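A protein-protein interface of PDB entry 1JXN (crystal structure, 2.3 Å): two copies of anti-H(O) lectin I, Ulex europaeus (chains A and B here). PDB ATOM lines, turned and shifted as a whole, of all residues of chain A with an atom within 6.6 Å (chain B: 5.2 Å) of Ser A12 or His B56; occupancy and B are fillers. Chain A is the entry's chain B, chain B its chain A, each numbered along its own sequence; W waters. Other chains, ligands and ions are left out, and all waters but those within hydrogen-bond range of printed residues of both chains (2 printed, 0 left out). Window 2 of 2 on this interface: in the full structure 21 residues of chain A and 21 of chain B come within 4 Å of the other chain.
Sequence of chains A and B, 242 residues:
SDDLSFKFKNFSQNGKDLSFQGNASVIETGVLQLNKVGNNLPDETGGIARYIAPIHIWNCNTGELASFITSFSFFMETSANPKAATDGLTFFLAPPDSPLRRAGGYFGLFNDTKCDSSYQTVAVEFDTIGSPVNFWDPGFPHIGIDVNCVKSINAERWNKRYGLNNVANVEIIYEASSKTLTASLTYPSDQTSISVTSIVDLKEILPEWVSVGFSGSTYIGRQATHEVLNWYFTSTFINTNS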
ATOM      1  N   PHE A   8       8.798  26.255   3.023  1.00  0.00           N
ATOM      2  CA  PHE A   8       8.436  25.067   2.288  1.00  0.00           C
ATOM      3  C   PHE A   8       9.326  25.097   1.059  1.00  0.00           C
ATOM      4  O   PHE A   8       9.283  26.073   0.304  1.00  0.00           O
ATOM      5  CB  PHE A   8       6.977  25.130   1.824  1.00  0.00           C
ATOM      6  CG  PHE A   8       5.963  25.012   2.927  1.00  0.00           C
ATOM      7  CD1 PHE A   8       5.378  23.785   3.216  1.00  0.00           C
ATOM      8  CD2 PHE A   8       5.550  26.134   3.635  1.00  0.00           C
ATOM      9  CE1 PHE A   8       4.393  23.675   4.188  1.00  0.00           C
ATOM     10  CE2 PHE A   8       4.568  26.037   4.609  1.00  0.00           C
ATOM     11  CZ  PHE A   8       3.985  24.804   4.887  1.00  0.00           C
ATOM     12  N   ASN A  10       9.222  22.630  -1.134  1.00  0.00           N
ATOM     13  CA  ASN A  10       8.353  21.893  -2.053  1.00  0.00           C
ATOM     14  C   ASN A  10       7.238  21.366  -1.148  1.00  0.00           C
ATOM     15  O   ASN A  10       7.258  21.635   0.053  1.00  0.00           O
ATOM     16  CB  ASN A  10       9.085  20.757  -2.799  1.00  0.00           C
ATOM     17  CG  ASN A  10       9.707  19.724  -1.859  1.00  0.00           C
ATOM     18  OD1 ASN A  10       9.003  19.024  -1.121  1.00  0.00           O
ATOM     19  ND2 ASN A  10      11.036  19.615  -1.898  1.00  0.00           N
ATOM     20  N   PHE A  11       6.297  20.594  -1.669  1.00  0.00           N
ATOM     21  CA  PHE A  11       5.196  20.152  -0.819  1.00  0.00           C
ATOM     22  C   PHE A  11       4.951  18.642  -0.689  1.00  0.00           C
ATOM     23  O   PHE A  11       5.111  17.885  -1.644  1.00  0.00           O
ATOM     24  CB  PHE A  11       3.930  20.899  -1.245  1.00  0.00           C
ATOM     25  CG  PHE A  11       4.080  22.395  -1.220  1.00  0.00           C
ATOM     26  CD1 PHE A  11       4.445  23.085  -2.370  1.00  0.00           C
ATOM     27  CD2 PHE A  11       3.888  23.112  -0.037  1.00  0.00           C
ATOM     28  CE1 PHE A  11       4.625  24.466  -2.347  1.00  0.00           C
ATOM     29  CE2 PHE A  11       4.064  24.498  -0.006  1.00  0.00           C
ATOM     30  CZ  PHE A  11       4.434  25.175  -1.167  1.00  0.00           C
ATOM     31  N   SER A  12       4.537  18.223   0.502  1.00  0.00           N
ATOM     32  CA  SER A  12       4.296  16.812   0.810  1.00  0.00           C
ATOM     33  C   SER A  12       2.950  16.307   0.348  1.00  0.00           C
ATOM     34  O   SER A  12       1.930  16.925   0.622  1.00  0.00           O
ATOM     35  CB  SER A  12       4.430  16.563   2.322  1.00  0.00           C
ATOM     36  OG  SER A  12       5.714  16.950   2.798  1.00  0.00           O
ATOM     37  N   GLN A  13       2.949  15.159  -0.322  1.00  0.00           N
ATOM     38  CA  GLN A  13       1.713  14.570  -0.815  1.00  0.00           C
ATOM     39  C   GLN A  13       0.702  14.393   0.311  1.00  0.00           C
ATOM     40  O   GLN A  13      -0.503  14.507   0.091  1.00  0.00           O
ATOM     41  CB  GLN A  13       1.991  13.231  -1.519  1.00  0.00           C
ATOM     42  CG  GLN A  13       1.673  13.219  -3.026  1.00  0.00           C
ATOM     43  CD  GLN A  13       0.182  13.194  -3.324  1.00  0.00           C
ATOM     44  OE1 GLN A  13      -0.333  12.235  -3.893  1.00  0.00           O
ATOM     45  NE2 GLN A  13      -0.516  14.261  -2.950  1.00  0.00           N
ATOM     46  N   ASN A  14       1.193  14.177   1.525  1.00  0.00           N
ATOM     47  CA  ASN A  14       0.307  13.995   2.672  1.00  0.00           C
ATOM     48  C   ASN A  14       0.651  14.905   3.853  1.00  0.00           C
ATOM     49  O   ASN A  14       0.706  14.479   5.017  1.00  0.00           O
ATOM     50  CB  ASN A  14       0.264  12.518   3.070  1.00  0.00           C
ATOM     51  CG  ASN A  14      -0.541  11.691   2.093  1.00  0.00           C
ATOM     52  OD1 ASN A  14      -1.753  11.886   1.975  1.00  0.00           O
ATOM     53  ND2 ASN A  14       0.127  10.808   1.341  1.00  0.00           N
ATOM     54  N   GLY A  15       0.787  16.190   3.543  1.00  0.00           N
ATOM     55  CA  GLY A  15       1.134  17.180   4.538  1.00  0.00           C
ATOM     56  C   GLY A  15       0.163  17.249   5.689  1.00  0.00           C
ATOM     57  O   GLY A  15      -0.933  16.718   5.612  1.00  0.00           O
ATOM     58  N   LYS A  16       0.557  17.935   6.754  1.00  0.00           N
ATOM     59  CA  LYS A  16      -0.300  18.048   7.929  1.00  0.00           C
ATOM     60  C   LYS A  16      -0.412  19.475   8.464  1.00  0.00           C
ATOM     61  O   LYS A  16      -1.234  19.758   9.342  1.00  0.00           O
ATOM     62  CB  LYS A  16       0.219  17.120   9.033  1.00  0.00           C
ATOM     63  CG  LYS A  16      -0.048  15.635   8.788  1.00  0.00           C
ATOM     64  CD  LYS A  16      -1.533  15.343   8.946  1.00  0.00           C
ATOM     65  CE  LYS A  16      -1.903  13.902   8.606  1.00  0.00           C
ATOM     66  NZ  LYS A  16      -3.388  13.725   8.710  1.00  0.00           N
ATOM     67  N   ASP A  17       0.370  20.382   7.888  1.00  0.00           N
ATOM     68  CA  ASP A  17       0.370  21.762   8.347  1.00  0.00           C
ATOM     69  C   ASP A  17      -0.291  22.780   7.428  1.00  0.00           C
ATOM     70  O   ASP A  17      -0.063  23.978   7.577  1.00  0.00           O
ATOM     71  CB  ASP A  17       1.796  22.207   8.693  1.00  0.00           C
ATOM     72  CG  ASP A  17       2.746  22.158   7.507  1.00  0.00           C
ATOM     73  OD1 ASP A  17       3.791  22.839   7.564  1.00  0.00           O
ATOM     74  OD2 ASP A  17       2.467  21.440   6.527  1.00  0.00           O
ATOM     75  N   PHE A  20      -6.773  23.216   3.408  1.00  0.00           N
ATOM     76  CA  PHE A  20      -7.216  23.312   2.025  1.00  0.00           C
ATOM     77  C   PHE A  20      -8.712  23.512   1.861  1.00  0.00           C
ATOM     78  O   PHE A  20      -9.526  22.772   2.426  1.00  0.00           O
ATOM     79  CB  PHE A  20      -6.798  22.074   1.229  1.00  0.00           C
ATOM     80  CG  PHE A  20      -5.319  21.861   1.167  1.00  0.00           C
ATOM     81  CD1 PHE A  20      -4.681  21.062   2.105  1.00  0.00           C
ATOM     82  CD2 PHE A  20      -4.563  22.443   0.165  1.00  0.00           C
ATOM     83  CE1 PHE A  20      -3.319  20.846   2.043  1.00  0.00           C
ATOM     84  CE2 PHE A  20      -3.190  22.227   0.099  1.00  0.00           C
ATOM     85  CZ  PHE A  20      -2.572  21.428   1.039  1.00  0.00           C
ATOM     86  N   VAL A  26      -1.934  19.421  -2.805  1.00  0.00           N
ATOM     87  CA  VAL A  26      -0.541  19.218  -3.169  1.00  0.00           C
ATOM     88  C   VAL A  26      -0.581  18.061  -4.156  1.00  0.00           C
ATOM     89  O   VAL A  26      -1.125  16.997  -3.855  1.00  0.00           O
ATOM     90  CB  VAL A  26       0.340  18.839  -1.962  1.00  0.00           C
ATOM     91  CG1 VAL A  26       1.767  18.584  -2.418  1.00  0.00           C
ATOM     92  CG2 VAL A  26       0.305  19.942  -0.912  1.00  0.00           C
ATOM     93  N   ILE A  27      -0.116  18.311  -5.373  1.00  0.00           N
ATOM     94  CA  ILE A  27      -0.118  17.270  -6.379  1.00  0.00           C
ATOM     95  C   ILE A  27       1.089  16.370  -6.173  1.00  0.00           C
ATOM     96  O   ILE A  27       2.113  16.777  -5.604  1.00  0.00           O
ATOM     97  CB  ILE A  27      -0.157  17.836  -7.819  1.00  0.00           C
ATOM     98  CG1 ILE A  27       0.939  18.882  -8.030  1.00  0.00           C
ATOM     99  CG2 ILE A  27      -1.522  18.386  -8.115  1.00  0.00           C
ATOM    100  CD1 ILE A  27       0.892  19.530  -9.394  1.00  0.00           C
ATOM    101  N   GLY A  30       4.770  17.159  -5.942  1.00  0.00           N
ATOM    102  CA  GLY A  30       5.276  17.962  -4.837  1.00  0.00           C
ATOM    103  C   GLY A  30       5.148  19.456  -5.033  1.00  0.00           C
ATOM    104  O   GLY A  30       5.993  20.217  -4.567  1.00  0.00           O
ATOM    105  N   VAL A  31       4.058  19.867  -5.673  1.00  0.00           N
ATOM    106  CA  VAL A  31       3.793  21.266  -5.984  1.00  0.00           C
ATOM    107  C   VAL A  31       2.443  21.671  -5.429  1.00  0.00           C
ATOM    108  O   VAL A  31       1.502  20.881  -5.447  1.00  0.00           O
ATOM    109  CB  VAL A  31       3.825  21.471  -7.526  1.00  0.00           C
ATOM    110  CG1 VAL A  31       2.851  22.540  -7.980  1.00  0.00           C
ATOM    111  CG2 VAL A  31       5.237  21.806  -7.961  1.00  0.00           C
ATOM    112  N   SER B   1       6.399  21.717   6.119  1.00  0.00           N
ATOM    113  CA  SER B   1       7.418  22.800   6.255  1.00  0.00           C
ATOM    114  C   SER B   1       8.767  22.134   6.446  1.00  0.00           C
ATOM    115  O   SER B   1       8.844  20.999   6.920  1.00  0.00           O
ATOM    116  CB  SER B   1       7.069  23.694   7.449  1.00  0.00           C
ATOM    117  OG  SER B   1       8.126  24.565   7.817  1.00  0.00           O
ATOM    118  N   PRO B  54       1.339  20.928  13.276  1.00  0.00           N
ATOM    119  CA  PRO B  54       2.202  19.747  13.375  1.00  0.00           C
ATOM    120  C   PRO B  54       3.523  20.010  12.661  1.00  0.00           C
ATOM    121  O   PRO B  54       3.543  20.615  11.587  1.00  0.00           O
ATOM    122  CB  PRO B  54       1.388  18.680  12.648  1.00  0.00           C
ATOM    123  CG  PRO B  54      -0.024  19.108  12.908  1.00  0.00           C
ATOM    124  CD  PRO B  54       0.050  20.584  12.664  1.00  0.00           C
ATOM    125  N   ILE B  55       4.620  19.584  13.293  1.00  0.00           N
ATOM    126  CA  ILE B  55       5.996  19.737  12.783  1.00  0.00           C
ATOM    127  C   ILE B  55       6.379  18.580  11.863  1.00  0.00           C
ATOM    128  O   ILE B  55       6.052  17.429  12.147  1.00  0.00           O
ATOM    129  CB  ILE B  55       7.032  19.704  13.942  1.00  0.00           C
ATOM    130  CG1 ILE B  55       6.559  20.543  15.130  1.00  0.00           C
ATOM    131  CG2 ILE B  55       8.404  20.171  13.447  1.00  0.00           C
ATOM    132  CD1 ILE B  55       6.581  22.027  14.909  1.00  0.00           C
ATOM    133  N   HIS B  56       7.113  18.888  10.795  1.00  0.00           N
ATOM    134  CA  HIS B  56       7.585  17.873   9.847  1.00  0.00           C
ATOM    135  C   HIS B  56       8.873  17.342  10.494  1.00  0.00           C
ATOM    136  O   HIS B  56       9.929  17.943  10.379  1.00  0.00           O
ATOM    137  CB  HIS B  56       7.883  18.524   8.484  1.00  0.00           C
ATOM    138  CG  HIS B  56       7.812  17.591   7.309  1.00  0.00           C
ATOM    139  ND1 HIS B  56       7.810  16.218   7.430  1.00  0.00           N
ATOM    140  CD2 HIS B  56       7.765  17.847   5.977  1.00  0.00           C
ATOM    141  CE1 HIS B  56       7.768  15.668   6.230  1.00  0.00           C
ATOM    142  NE2 HIS B  56       7.741  16.639   5.329  1.00  0.00           N
ATOM    143  N   ILE B  57       8.762  16.236  11.221  1.00  0.00           N
ATOM    144  CA  ILE B  57       9.910  15.682  11.926  1.00  0.00           C
ATOM    145  C   ILE B  57      10.881  14.905  11.050  1.00  0.00           C
ATOM    146  O   ILE B  57      12.089  15.083  11.179  1.00  0.00           O
ATOM    147  CB  ILE B  57       9.464  14.874  13.188  1.00  0.00           C
ATOM    148  CG1 ILE B  57      10.586  14.855  14.229  1.00  0.00           C
ATOM    149  CG2 ILE B  57       8.967  13.481  12.824  1.00  0.00           C
ATOM    150  CD1 ILE B  57      10.844  16.217  14.854  1.00  0.00           C
ATOM    151  N   TRP B  58      10.375  14.072  10.143  1.00  0.00           N
ATOM    152  CA  TRP B  58      11.263  13.322   9.240  1.00  0.00           C
ATOM    153  C   TRP B  58      10.640  13.073   7.875  1.00  0.00           C
ATOM    154  O   TRP B  58       9.432  12.908   7.773  1.00  0.00           O
ATOM    155  CB  TRP B  58      11.770  12.010   9.875  1.00  0.00           C
ATOM    156  CG  TRP B  58      10.743  10.956  10.159  1.00  0.00           C
ATOM    157  CD1 TRP B  58      10.047  10.782  11.321  1.00  0.00           C
ATOM    158  CD2 TRP B  58      10.375   9.866   9.303  1.00  0.00           C
ATOM    159  NE1 TRP B  58       9.281   9.646  11.250  1.00  0.00           N
ATOM    160  CE2 TRP B  58       9.459   9.064  10.021  1.00  0.00           C
ATOM    161  CE3 TRP B  58      10.736   9.484   8.008  1.00  0.00           C
ATOM    162  CZ2 TRP B  58       8.899   7.901   9.484  1.00  0.00           C
ATOM    163  CZ3 TRP B  58      10.181   8.329   7.473  1.00  0.00           C
ATOM    164  CH2 TRP B  58       9.273   7.552   8.211  1.00  0.00           C
ATOM    165  N   ASN B  59      11.469  13.031   6.837  1.00  0.00           N
ATOM    166  CA  ASN B  59      10.981  12.838   5.472  1.00  0.00           C
ATOM    167  C   ASN B  59      11.177  11.411   4.984  1.00  0.00           C
ATOM    168  O   ASN B  59      12.304  10.973   4.767  1.00  0.00           O
ATOM    169  CB  ASN B  59      11.678  13.833   4.522  1.00  0.00           C
ATOM    170  CG  ASN B  59      11.034  13.884   3.119  1.00  0.00           C
ATOM    171  OD1 ASN B  59      10.963  12.884   2.397  1.00  0.00           O
ATOM    172  ND2 ASN B  59      10.592  15.079   2.726  1.00  0.00           N
ATOM    173  N   ALA B  66      15.143  16.055  10.712  1.00  0.00           N
ATOM    174  CA  ALA B  66      15.249  17.454  11.119  1.00  0.00           C
ATOM    175  C   ALA B  66      15.835  17.657  12.503  1.00  0.00           C
ATOM    176  O   ALA B  66      15.405  17.023  13.475  1.00  0.00           O
ATOM    177  CB  ALA B  66      13.890  18.123  11.044  1.00  0.00           C
ATOM    178  N   GLU B 208       5.815  10.751  10.797  1.00  0.00           N
ATOM    179  CA  GLU B 208       6.304  11.799   9.893  1.00  0.00           C
ATOM    180  C   GLU B 208       6.075  13.220  10.390  1.00  0.00           C
ATOM    181  O   GLU B 208       6.950  14.079  10.258  1.00  0.00           O
ATOM    182  CB  GLU B 208       5.688  11.639   8.502  1.00  0.00           C
ATOM    183  CG  GLU B 208       6.116  10.368   7.787  1.00  0.00           C
ATOM    184  CD  GLU B 208       6.231  10.579   6.298  1.00  0.00           C
ATOM    185  OE1 GLU B 208       7.013  11.465   5.889  1.00  0.00           O
ATOM    186  OE2 GLU B 208       5.536   9.873   5.535  1.00  0.00           O
ATOM    187  N   TRP B 209       4.919  13.447  10.995  1.00  0.00           N
ATOM    188  CA  TRP B 209       4.564  14.753  11.518  1.00  0.00           C
ATOM    189  C   TRP B 209       4.200  14.581  12.984  1.00  0.00           C
ATOM    190  O   TRP B 209       3.527  13.623  13.356  1.00  0.00           O
ATOM    191  CB  TRP B 209       3.374  15.351  10.744  1.00  0.00           C
ATOM    192  CG  TRP B 209       3.583  15.481   9.230  1.00  0.00           C
ATOM    193  CD1 TRP B 209       3.565  14.470   8.301  1.00  0.00           C
ATOM    194  CD2 TRP B 209       3.812  16.690   8.498  1.00  0.00           C
ATOM    195  NE1 TRP B 209       3.766  14.977   7.042  1.00  0.00           N
ATOM    196  CE2 TRP B 209       3.920  16.340   7.130  1.00  0.00           C
ATOM    197  CE3 TRP B 209       3.934  18.040   8.855  1.00  0.00           C
ATOM    198  CZ2 TRP B 209       4.144  17.280   6.127  1.00  0.00           C
ATOM    199  CZ3 TRP B 209       4.155  18.981   7.858  1.00  0.00           C
ATOM    200  CH2 TRP B 209       4.257  18.591   6.505  1.00  0.00           C
ATOM    201  N   VAL B 210       4.674  15.486  13.821  1.00  0.00           N
ATOM    202  CA  VAL B 210       4.386  15.413  15.243  1.00  0.00           C
ATOM    203  C   VAL B 210       4.055  16.774  15.813  1.00  0.00           C
ATOM    204  O   VAL B 210       4.243  17.797  15.171  1.00  0.00           O
ATOM    205  CB  VAL B 210       5.598  14.901  16.046  1.00  0.00           C
ATOM    206  CG1 VAL B 210       5.863  13.433  15.763  1.00  0.00           C
ATOM    207  CG2 VAL B 210       6.820  15.764  15.763  1.00  0.00           C
ATOM    208  N   PHE B 237      15.196  20.676   8.414  1.00  0.00           N
ATOM    209  CA  PHE B 237      15.655  19.477   7.744  1.00  0.00           C
ATOM    210  C   PHE B 237      16.951  19.758   7.051  1.00  0.00           C
ATOM    211  O   PHE B 237      17.698  18.835   6.728  1.00  0.00           O
ATOM    212  CB  PHE B 237      14.668  19.071   6.676  1.00  0.00           C
ATOM    213  CG  PHE B 237      13.676  18.081   7.127  1.00  0.00           C
ATOM    214  CD1 PHE B 237      14.026  16.749   7.239  1.00  0.00           C
ATOM    215  CD2 PHE B 237      12.375  18.466   7.391  1.00  0.00           C
ATOM    216  CE1 PHE B 237      13.090  15.815   7.603  1.00  0.00           C
ATOM    217  CE2 PHE B 237      11.426  17.532   7.758  1.00  0.00           C
ATOM    218  CZ  PHE B 237      11.781  16.205   7.863  1.00  0.00           C
HETATM  219  O   HOH W   1       8.015  20.714   3.258  1.00  0.00           O
HETATM  220  O   HOH W   2       3.886  13.969   4.198  1.00  0.00           O
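The side-chain carboxylate (OD1) of Asp A17 is in hydrogen-bond range of the backbone NH (N) of Ser B1, at 3.2 Å. OG of Ser A12 lies within hydrogen-bond range of NE2 of His B56.
Among the printed residues, pairs that only touch across the chains: Phe A8 with Ser B1, Ser A12 with Trp B209, Asn A14 with Trp B209, Gly A15 with Trp B209, Lys A16 with Pro B54, Lys A16 with Trp B209, Asp A17 with Pro B54 and Asp A17 with Trp B209.
Phe A11 touches none of the printed residues of chain B. Ser A12 touches two residues of chain B. Of the printed residues of chain B, Gly A15 touches Trp B209. Of the printed residues of chain B, Lys A16 touches Pro B54 (3.7 Å) and Trp B209 (3.7 Å). Of the printed residues of chain B, Asp A17 touches Ser B1 (3.2 Å), Pro B54 (3.7 Å) and Trp B209 (3.3 Å). His B56 touches just one residue of chain A: Ser A12. Trp B58 touches none of the printed residues of chain A. Printed residues of chain A within 4 Å of Trp B209: Ser A12 (3.7 Å), Asn A14 (3.7 Å), Gly A15 (3.4 Å), Lys A16 (3.7 Å) and Asp A17 (3.3 Å). The nearest printed residue of chain B that does not touch Ser A12 is Asn B59 (5.2 Å). The nearest residue of chain A that does not touch His B56 is Asp A17 (6.0 Å).
Of the 12 printed residues of chain B, 4 touch a printed residue of chain A. Among the printed residues, no Asp or Glu carboxylate lies within 4 Å of a Lys or Arg side-chain nitrogen of the other chain.
No position is printed for both chains. Of the 10 pairs that touch across the chains among the printed residues, none has its exchanged pair printed and touching as well.
Water W2 lies within hydrogen-bond range of the indole nitrogen (NE1) of Trp B209 (3.0 Å) and the backbone carbonyl oxygen (O) of Asn A14 (3.3 Å). Water W1 bridges O of Asn A10 (3.4 Å) and N of Ser B1 (3.4 Å).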
